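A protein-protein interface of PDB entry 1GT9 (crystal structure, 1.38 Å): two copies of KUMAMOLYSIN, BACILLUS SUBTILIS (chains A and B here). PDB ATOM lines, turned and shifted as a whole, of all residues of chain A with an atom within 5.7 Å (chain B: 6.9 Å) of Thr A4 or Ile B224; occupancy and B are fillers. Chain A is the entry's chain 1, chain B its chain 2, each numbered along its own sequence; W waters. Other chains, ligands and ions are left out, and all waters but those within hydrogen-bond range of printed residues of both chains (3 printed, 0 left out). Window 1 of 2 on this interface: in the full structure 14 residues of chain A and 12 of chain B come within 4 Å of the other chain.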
ATOM      1  N   ALA A   2     -19.595  20.477   5.968  1.00  0.00           N
ATOM      2  CA  ALA A   2     -20.809  20.785   6.716  1.00  0.00           C
ATOM      3  C   ALA A   2     -21.884  21.313   5.771  1.00  0.00           C
ATOM      4  O   ALA A   2     -21.594  22.164   4.929  1.00  0.00           O
ATOM      5  CB  ALA A   2     -20.519  21.826   7.808  1.00  0.00           C
ATOM      6  N   PRO A   3     -23.122  20.797   5.870  1.00  0.00           N
ATOM      7  CA  PRO A   3     -24.178  21.302   4.973  1.00  0.00           C
ATOM      8  C   PRO A   3     -24.474  22.772   5.267  1.00  0.00           C
ATOM      9  O   PRO A   3     -24.430  23.219   6.430  1.00  0.00           O
ATOM     10  CB  PRO A   3     -25.380  20.390   5.280  1.00  0.00           C
ATOM     11  CG  PRO A   3     -25.072  19.853   6.666  1.00  0.00           C
ATOM     12  CD  PRO A   3     -23.590  19.604   6.605  1.00  0.00           C
ATOM     13  N   THR A   4     -24.772  23.519   4.208  1.00  0.00           N
ATOM     14  CA  THR A   4     -25.077  24.925   4.314  1.00  0.00           C
ATOM     15  C   THR A   4     -26.283  25.250   3.455  1.00  0.00           C
ATOM     16  O   THR A   4     -26.842  24.383   2.780  1.00  0.00           O
ATOM     17  CB  THR A   4     -23.886  25.789   3.872  1.00  0.00           C
ATOM     18  OG1 THR A   4     -23.573  25.519   2.490  1.00  0.00           O
ATOM     19  CG2 THR A   4     -22.657  25.482   4.716  1.00  0.00           C
ATOM     20  N   ALA A   5     -26.705  26.498   3.497  1.00  0.00           N
ATOM     21  CA  ALA A   5     -27.848  26.928   2.713  1.00  0.00           C
ATOM     22  C   ALA A   5     -27.711  28.429   2.510  1.00  0.00           C
ATOM     23  O   ALA A   5     -27.010  29.125   3.273  1.00  0.00           O
ATOM     24  CB  ALA A   5     -29.157  26.600   3.432  1.00  0.00           C
ATOM     25  N   TYR A   6     -28.357  28.901   1.454  1.00  0.00           N
ATOM     26  CA  TYR A   6     -28.347  30.306   1.084  1.00  0.00           C
ATOM     27  C   TYR A   6     -29.758  30.797   0.872  1.00  0.00           C
ATOM     28  O   TYR A   6     -30.640  30.019   0.529  1.00  0.00           O
ATOM     29  CB  TYR A   6     -27.673  30.518  -0.287  1.00  0.00           C
ATOM     30  CG  TYR A   6     -26.270  30.020  -0.410  1.00  0.00           C
ATOM     31  CD1 TYR A   6     -25.965  28.898  -1.177  1.00  0.00           C
ATOM     32  CD2 TYR A   6     -25.236  30.689   0.226  1.00  0.00           C
ATOM     33  CE1 TYR A   6     -24.645  28.452  -1.316  1.00  0.00           C
ATOM     34  CE2 TYR A   6     -23.924  30.245   0.111  1.00  0.00           C
ATOM     35  CZ  TYR A   6     -23.637  29.130  -0.664  1.00  0.00           C
ATOM     36  OH  TYR A   6     -22.338  28.696  -0.796  1.00  0.00           O
ATOM     37  N   LEU A 195     -22.163  25.323  -5.053  1.00  0.00           N
ATOM     38  CA  LEU A 195     -21.607  26.669  -4.957  1.00  0.00           C
ATOM     39  C   LEU A 195     -21.179  27.038  -3.547  1.00  0.00           C
ATOM     40  O   LEU A 195     -21.979  26.919  -2.615  1.00  0.00           O
ATOM     41  CB  LEU A 195     -22.669  27.679  -5.427  1.00  0.00           C
ATOM     42  CG  LEU A 195     -22.247  29.148  -5.338  1.00  0.00           C
ATOM     43  CD1 LEU A 195     -21.212  29.432  -6.413  1.00  0.00           C
ATOM     44  CD2 LEU A 195     -23.465  30.059  -5.489  1.00  0.00           C
ATOM     45  N   PRO A 259     -28.220  20.205  -2.757  1.00  0.00           N
ATOM     46  CA  PRO A 259     -28.996  20.415  -1.517  1.00  0.00           C
ATOM     47  C   PRO A 259     -28.082  20.710  -0.315  1.00  0.00           C
ATOM     48  O   PRO A 259     -28.512  21.394   0.626  1.00  0.00           O
ATOM     49  CB  PRO A 259     -29.774  19.107  -1.363  1.00  0.00           C
ATOM     50  CG  PRO A 259     -29.983  18.654  -2.802  1.00  0.00           C
ATOM     51  CD  PRO A 259     -28.587  18.950  -3.425  1.00  0.00           C
ATOM     52  N   ALA A 260     -26.844  20.195  -0.350  1.00  0.00           N
ATOM     53  CA  ALA A 260     -25.884  20.444   0.726  1.00  0.00           C
ATOM     54  C   ALA A 260     -25.347  21.886   0.769  1.00  0.00           C
ATOM     55  O   ALA A 260     -24.644  22.250   1.704  1.00  0.00           O
ATOM     56  CB  ALA A 260     -24.719  19.406   0.670  1.00  0.00           C
ATOM     57  N   THR A 261     -25.664  22.693  -0.254  1.00  0.00           N
ATOM     58  CA  THR A 261     -25.346  24.138  -0.331  1.00  0.00           C
ATOM     59  C   THR A 261     -26.629  24.728  -0.935  1.00  0.00           C
ATOM     60  O   THR A 261     -26.610  25.623  -1.789  1.00  0.00           O
ATOM     61  CB  THR A 261     -24.134  24.489  -1.259  1.00  0.00           C
ATOM     62  OG1 THR A 261     -24.348  24.014  -2.603  1.00  0.00           O
ATOM     63  CG2 THR A 261     -22.852  23.890  -0.728  1.00  0.00           C
ATOM     64  N   GLY A 262     -27.756  24.225  -0.435  1.00  0.00           N
ATOM     65  CA  GLY A 262     -29.065  24.545  -0.980  1.00  0.00           C
ATOM     66  C   GLY A 262     -29.728  25.859  -0.708  1.00  0.00           C
ATOM     67  O   GLY A 262     -29.097  26.788  -0.228  1.00  0.00           O
ATOM     68  N   VAL A 273     -34.519  23.466   3.642  1.00  0.00           N
ATOM     69  CA  VAL A 273     -33.578  23.616   2.547  1.00  0.00           C
ATOM     70  C   VAL A 273     -33.961  22.670   1.424  1.00  0.00           C
ATOM     71  O   VAL A 273     -34.245  21.479   1.653  1.00  0.00           O
ATOM     72  CB  VAL A 273     -32.142  23.267   3.011  1.00  0.00           C
ATOM     73  CG1 VAL A 273     -31.149  23.456   1.839  1.00  0.00           C
ATOM     74  CG2 VAL A 273     -31.743  24.185   4.176  1.00  0.00           C
ATOM     75  N   GLU B 133     -22.137  26.140  15.543  1.00  0.00           N
ATOM     76  CA  GLU B 133     -22.660  26.499  14.224  1.00  0.00           C
ATOM     77  C   GLU B 133     -23.165  25.305  13.425  1.00  0.00           C
ATOM     78  O   GLU B 133     -24.102  25.468  12.647  1.00  0.00           O
ATOM     79  CB  GLU B 133     -21.596  27.260  13.398  1.00  0.00           C
ATOM     80  CG  GLU B 133     -20.419  26.387  13.039  1.00  0.00           C
ATOM     81  CD  GLU B 133     -19.418  27.022  12.104  1.00  0.00           C
ATOM     82  OE1 GLU B 133     -19.591  28.191  11.665  1.00  0.00           O
ATOM     83  OE2 GLU B 133     -18.436  26.311  11.844  1.00  0.00           O
ATOM     84  N   ASP B 134     -22.558  24.136  13.623  1.00  0.00           N
ATOM     85  CA  ASP B 134     -22.927  22.928  12.894  1.00  0.00           C
ATOM     86  C   ASP B 134     -23.962  22.062  13.608  1.00  0.00           C
ATOM     87  O   ASP B 134     -24.260  20.959  13.146  1.00  0.00           O
ATOM     88  CB  ASP B 134     -21.661  22.123  12.592  1.00  0.00           C
ATOM     89  CG  ASP B 134     -20.632  22.221  13.717  1.00  0.00           C
ATOM     90  OD1 ASP B 134     -21.040  22.467  14.871  1.00  0.00           O
ATOM     91  OD2 ASP B 134     -19.426  22.061  13.452  1.00  0.00           O
ATOM     92  N   PRO B 138     -29.320  23.982   8.834  1.00  0.00           N
ATOM     93  CA  PRO B 138     -28.779  24.922   7.838  1.00  0.00           C
ATOM     94  C   PRO B 138     -29.723  26.031   7.411  1.00  0.00           C
ATOM     95  O   PRO B 138     -29.281  27.147   7.164  1.00  0.00           O
ATOM     96  CB  PRO B 138     -28.355  24.008   6.677  1.00  0.00           C
ATOM     97  CG  PRO B 138     -27.880  22.774   7.418  1.00  0.00           C
ATOM     98  CD  PRO B 138     -29.015  22.588   8.469  1.00  0.00           C
ATOM     99  N   ALA B 139     -31.022  25.768   7.350  1.00  0.00           N
ATOM    100  CA  ALA B 139     -31.954  26.790   6.971  1.00  0.00           C
ATOM    101  C   ALA B 139     -32.003  27.909   8.010  1.00  0.00           C
ATOM    102  O   ALA B 139     -32.204  29.081   7.659  1.00  0.00           O
ATOM    103  CB  ALA B 139     -33.319  26.166   6.783  1.00  0.00           C
ATOM    104  N   ILE B 141     -29.444  28.788  10.006  1.00  0.00           N
ATOM    105  CA  ILE B 141     -28.190  29.521   9.869  1.00  0.00           C
ATOM    106  C   ILE B 141     -28.343  30.501   8.709  1.00  0.00           C
ATOM    107  O   ILE B 141     -27.950  31.657   8.815  1.00  0.00           O
ATOM    108  CB  ILE B 141     -27.011  28.582   9.536  1.00  0.00           C
ATOM    109  CG1 ILE B 141     -26.695  27.689  10.737  1.00  0.00           C
ATOM    110  CG2 ILE B 141     -25.801  29.429   9.101  1.00  0.00           C
ATOM    111  CD1 ILE B 141     -26.227  28.466  11.977  1.00  0.00           C
ATOM    112  N   ALA B 142     -28.895  30.045   7.590  1.00  0.00           N
ATOM    113  CA  ALA B 142     -29.080  30.929   6.442  1.00  0.00           C
ATOM    114  C   ALA B 142     -29.995  32.116   6.779  1.00  0.00           C
ATOM    115  O   ALA B 142     -29.702  33.270   6.450  1.00  0.00           O
ATOM    116  CB  ALA B 142     -29.661  30.126   5.254  1.00  0.00           C
ATOM    117  N   VAL B 178     -16.984  26.094  16.287  1.00  0.00           N
ATOM    118  CA  VAL B 178     -17.187  27.480  16.664  1.00  0.00           C
ATOM    119  C   VAL B 178     -18.683  27.703  16.858  1.00  0.00           C
ATOM    120  O   VAL B 178     -19.532  26.995  16.283  1.00  0.00           O
ATOM    121  CB  VAL B 178     -16.625  28.505  15.659  1.00  0.00           C
ATOM    122  CG1 VAL B 178     -15.113  28.374  15.644  1.00  0.00           C
ATOM    123  CG2 VAL B 178     -17.227  28.313  14.271  1.00  0.00           C
ATOM    124  N   PHE B 180     -22.332  29.869  16.939  1.00  0.00           N
ATOM    125  CA  PHE B 180     -23.131  30.765  16.091  1.00  0.00           C
ATOM    126  C   PHE B 180     -24.122  31.376  17.100  1.00  0.00           C
ATOM    127  O   PHE B 180     -24.660  30.655  17.967  1.00  0.00           O
ATOM    128  CB  PHE B 180     -23.834  29.949  14.998  1.00  0.00           C
ATOM    129  CG  PHE B 180     -24.598  30.785  14.025  1.00  0.00           C
ATOM    130  CD1 PHE B 180     -23.963  31.395  12.940  1.00  0.00           C
ATOM    131  CD2 PHE B 180     -25.952  31.016  14.229  1.00  0.00           C
ATOM    132  CE1 PHE B 180     -24.654  32.231  12.072  1.00  0.00           C
ATOM    133  CE2 PHE B 180     -26.653  31.860  13.357  1.00  0.00           C
ATOM    134  CZ  PHE B 180     -25.979  32.469  12.271  1.00  0.00           C
ATOM    135  N   ALA B 183     -20.071  33.072  14.673  1.00  0.00           N
ATOM    136  CA  ALA B 183     -19.427  32.704  13.416  1.00  0.00           C
ATOM    137  C   ALA B 183     -19.897  33.492  12.204  1.00  0.00           C
ATOM    138  O   ALA B 183     -19.180  33.560  11.202  1.00  0.00           O
ATOM    139  CB  ALA B 183     -19.579  31.206  13.160  1.00  0.00           C
ATOM    140  N   VAL B 221     -12.082  28.217  13.648  1.00  0.00           N
ATOM    141  CA  VAL B 221     -12.242  28.459  12.211  1.00  0.00           C
ATOM    142  C   VAL B 221     -13.566  27.867  11.755  1.00  0.00           C
ATOM    143  O   VAL B 221     -13.826  26.670  11.919  1.00  0.00           O
ATOM    144  CB  VAL B 221     -11.086  27.781  11.430  1.00  0.00           C
ATOM    145  CG1 VAL B 221     -11.251  28.056   9.907  1.00  0.00           C
ATOM    146  CG2 VAL B 221      -9.734  28.291  11.953  1.00  0.00           C
ATOM    147  N   SER B 222     -14.424  28.709  11.189  1.00  0.00           N
ATOM    148  CA  SER B 222     -15.733  28.220  10.757  1.00  0.00           C
ATOM    149  C   SER B 222     -15.674  27.146   9.680  1.00  0.00           C
ATOM    150  O   SER B 222     -14.822  27.189   8.803  1.00  0.00           O
ATOM    151  CB  SER B 222     -16.587  29.388  10.258  1.00  0.00           C
ATOM    152  OG  SER B 222     -17.855  28.920   9.809  1.00  0.00           O
ATOM    153  N   ARG B 223     -16.595  26.183   9.766  1.00  0.00           N
ATOM    154  CA  ARG B 223     -16.739  25.101   8.776  1.00  0.00           C
ATOM    155  C   ARG B 223     -17.845  25.491   7.812  1.00  0.00           C
ATOM    156  O   ARG B 223     -18.093  24.795   6.833  1.00  0.00           O
ATOM    157  CB  ARG B 223     -17.241  23.799   9.447  1.00  0.00           C
ATOM    158  CG  ARG B 223     -16.417  23.221  10.565  1.00  0.00           C
ATOM    159  CD  ARG B 223     -17.119  21.969  11.160  1.00  0.00           C
ATOM    160  N   ILE B 224     -18.503  26.604   8.097  1.00  0.00           N
ATOM    161  CA  ILE B 224     -19.658  27.058   7.327  1.00  0.00           C
ATOM    162  C   ILE B 224     -19.447  28.306   6.491  1.00  0.00           C
ATOM    163  O   ILE B 224     -19.787  28.373   5.298  1.00  0.00           O
ATOM    164  CB  ILE B 224     -20.848  27.240   8.199  1.00  0.00           C
ATOM    165  CG1 ILE B 224     -21.223  25.971   8.968  1.00  0.00           C
ATOM    166  CG2 ILE B 224     -21.985  27.996   7.469  1.00  0.00           C
ATOM    167  CD1 ILE B 224     -21.867  24.991   8.054  1.00  0.00           C
ATOM    168  N   PHE B 225     -18.802  29.303   7.082  1.00  0.00           N
ATOM    169  CA  PHE B 225     -18.551  30.568   6.413  1.00  0.00           C
ATOM    170  C   PHE B 225     -17.159  30.710   5.889  1.00  0.00           C
ATOM    171  O   PHE B 225     -16.192  30.497   6.621  1.00  0.00           O
ATOM    172  CB  PHE B 225     -18.836  31.713   7.376  1.00  0.00           C
ATOM    173  CG  PHE B 225     -20.263  31.730   7.887  1.00  0.00           C
ATOM    174  CD1 PHE B 225     -20.569  31.251   9.156  1.00  0.00           C
ATOM    175  CD2 PHE B 225     -21.304  32.181   7.060  1.00  0.00           C
ATOM    176  CE1 PHE B 225     -21.893  31.231   9.584  1.00  0.00           C
ATOM    177  CE2 PHE B 225     -22.618  32.157   7.482  1.00  0.00           C
ATOM    178  CZ  PHE B 225     -22.909  31.680   8.751  1.00  0.00           C
ATOM    179  N   PRO B 226     -17.026  31.025   4.591  1.00  0.00           N
ATOM    180  CA  PRO B 226     -15.683  31.190   4.026  1.00  0.00           C
ATOM    181  C   PRO B 226     -14.946  32.339   4.723  1.00  0.00           C
ATOM    182  O   PRO B 226     -15.560  33.210   5.333  1.00  0.00           O
ATOM    183  CB  PRO B 226     -15.949  31.564   2.572  1.00  0.00           C
ATOM    184  CG  PRO B 226     -17.291  30.982   2.281  1.00  0.00           C
ATOM    185  CD  PRO B 226     -18.077  31.176   3.576  1.00  0.00           C
ATOM    186  N   SER B 246     -10.258  26.420   5.026  1.00  0.00           N
ATOM    187  CA  SER B 246     -10.125  27.835   5.320  1.00  0.00           C
ATOM    188  C   SER B 246     -11.536  28.260   5.695  1.00  0.00           C
ATOM    189  O   SER B 246     -12.509  27.749   5.141  1.00  0.00           O
ATOM    190  CB  SER B 246      -9.662  28.579   4.064  1.00  0.00           C
ATOM    191  OG  SER B 246      -9.297  29.921   4.331  1.00  0.00           O
ATOM    192  N   GLY B 247     -11.667  29.161   6.650  1.00  0.00           N
ATOM    193  CA  GLY B 247     -12.989  29.630   7.015  1.00  0.00           C
ATOM    194  C   GLY B 247     -12.863  30.878   7.866  1.00  0.00           C
ATOM    195  O   GLY B 247     -11.749  31.277   8.273  1.00  0.00           O
ATOM    196  N   ARG B 248     -13.995  31.517   8.106  1.00  0.00           N
ATOM    197  CA  ARG B 248     -14.076  32.723   8.946  1.00  0.00           C
ATOM    198  C   ARG B 248     -13.488  32.432  10.330  1.00  0.00           C
ATOM    199  O   ARG B 248     -13.873  31.463  11.002  1.00  0.00           O
ATOM    200  CB  ARG B 248     -15.555  33.130   9.019  1.00  0.00           C
ATOM    201  CG  ARG B 248     -15.919  34.436   9.745  1.00  0.00           C
ATOM    202  CD  ARG B 248     -16.125  34.253  11.259  1.00  0.00           C
ATOM    203  NE  ARG B 248     -16.913  35.348  11.839  1.00  0.00           N
ATOM    204  CZ  ARG B 248     -16.429  36.493  12.325  1.00  0.00           C
ATOM    205  NH1 ARG B 248     -15.115  36.748  12.354  1.00  0.00           N
ATOM    206  NH2 ARG B 248     -17.282  37.450  12.684  1.00  0.00           N
HETATM  207  O   HOH W   1     -17.118  22.292   6.107  1.00  0.00           O
HETATM  208  O   HOH W   2     -19.494  23.971   4.524  1.00  0.00           O
HETATM  209  O   HOH W   3     -26.395  27.420   6.298  1.00  0.00           O
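The backbone NH of Thr A4 is in hydrogen-bond range of the backbone carbonyl oxygen of Ala A260 (2.8 Å). The backbone carbonyl oxygen of Thr A4 is in hydrogen-bond range of the backbone NH of Gly A262 (3.3 Å). The side-chain carboxylate (OE2) of Glu B133 is in hydrogen-bond range of the backbone NH (N) of Arg B223, at 2.8 Å. The side-chain hydroxyl (OG) of Ser B222 lies within hydrogen-bond range of the backbone NH (N) of Ile B224 (3.0 Å).
Among the printed residues, pairs that only touch across the chains: Ala A2 with Arg B223 (3.96 Å), Ala A2 with Ile B224 (3.4 Å), Pro A3 with Pro B138 (3.6 Å), Pro A3 with Ile B224 (3.5 Å), Thr A4 with Ile B224 (3.5 Å), Ala A5 with Pro B138 (3.8 Å), Ala A5 with Ala B142 (3.5 Å) and Val A273 with Ala B139 (3.6 Å).
Of the printed residues of chain B, Pro A3 touches Pro B138 and Ile B224. Of the printed residues of chain B, Thr A4 touches Ile B224 (3.5 Å). Of the printed residues of chain B, Ala A5 touches Pro B138 (3.8 Å) and Ala B142 (3.5 Å). Tyr A6 touches none of the printed residues of chain B. Printed residues of chain A within 4 Å of Arg B223: Ala A2 (3.96 Å). Printed residues of chain A within 4 Å of Ile B224: Ala A2 (3.4 Å), Pro A3 (3.5 Å) and Thr A4 (3.5 Å). Gly B247 touches none of the printed residues of chain A. The nearest printed residue of chain B that does not touch Thr A4 is Pro B138 (4.03 Å). The nearest printed residue of chain A that does not touch Ile B224 is Ala A5 (6.3 Å).
Of the 11 printed residues of chain A, 5 touch a printed residue of chain B. Printed residues of chain A that touch a printed residue of chain B: Ala A2, Pro A3, Thr A4, Ala A5 and Val A273. Hydrophobic or aromatic side chains of chain A that line the printed part of chain B: Ala A2, Ala A5 and Val A273. Of the 18 printed residues of chain B, 5 touch a printed residue of chain A. Printed residues of chain B that touch a printed residue of chain A: Pro B138, Ala B139, Ala B142, Arg B223 and Ile B224.
No position is printed for both chains. Of the 8 pairs that touch across the chains among the printed residues, none has its exchanged pair printed and touching as well.
Water W1 lies within hydrogen-bond range of the backbone carbonyl oxygen of Arg B223 (2.8 Å) and the backbone NH of Ala A2 (3.1 Å). Water W2 bridges the backbone carbonyl oxygen (O) of Ala A2 (2.8 Å) and the backbone carbonyl oxygen (O) of Arg B223 (2.8 Å). Water W3 bridges the backbone NH of Ala A5 (3.0 Å) and the backbone carbonyl oxygen of Pro B138 (3.0 Å).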
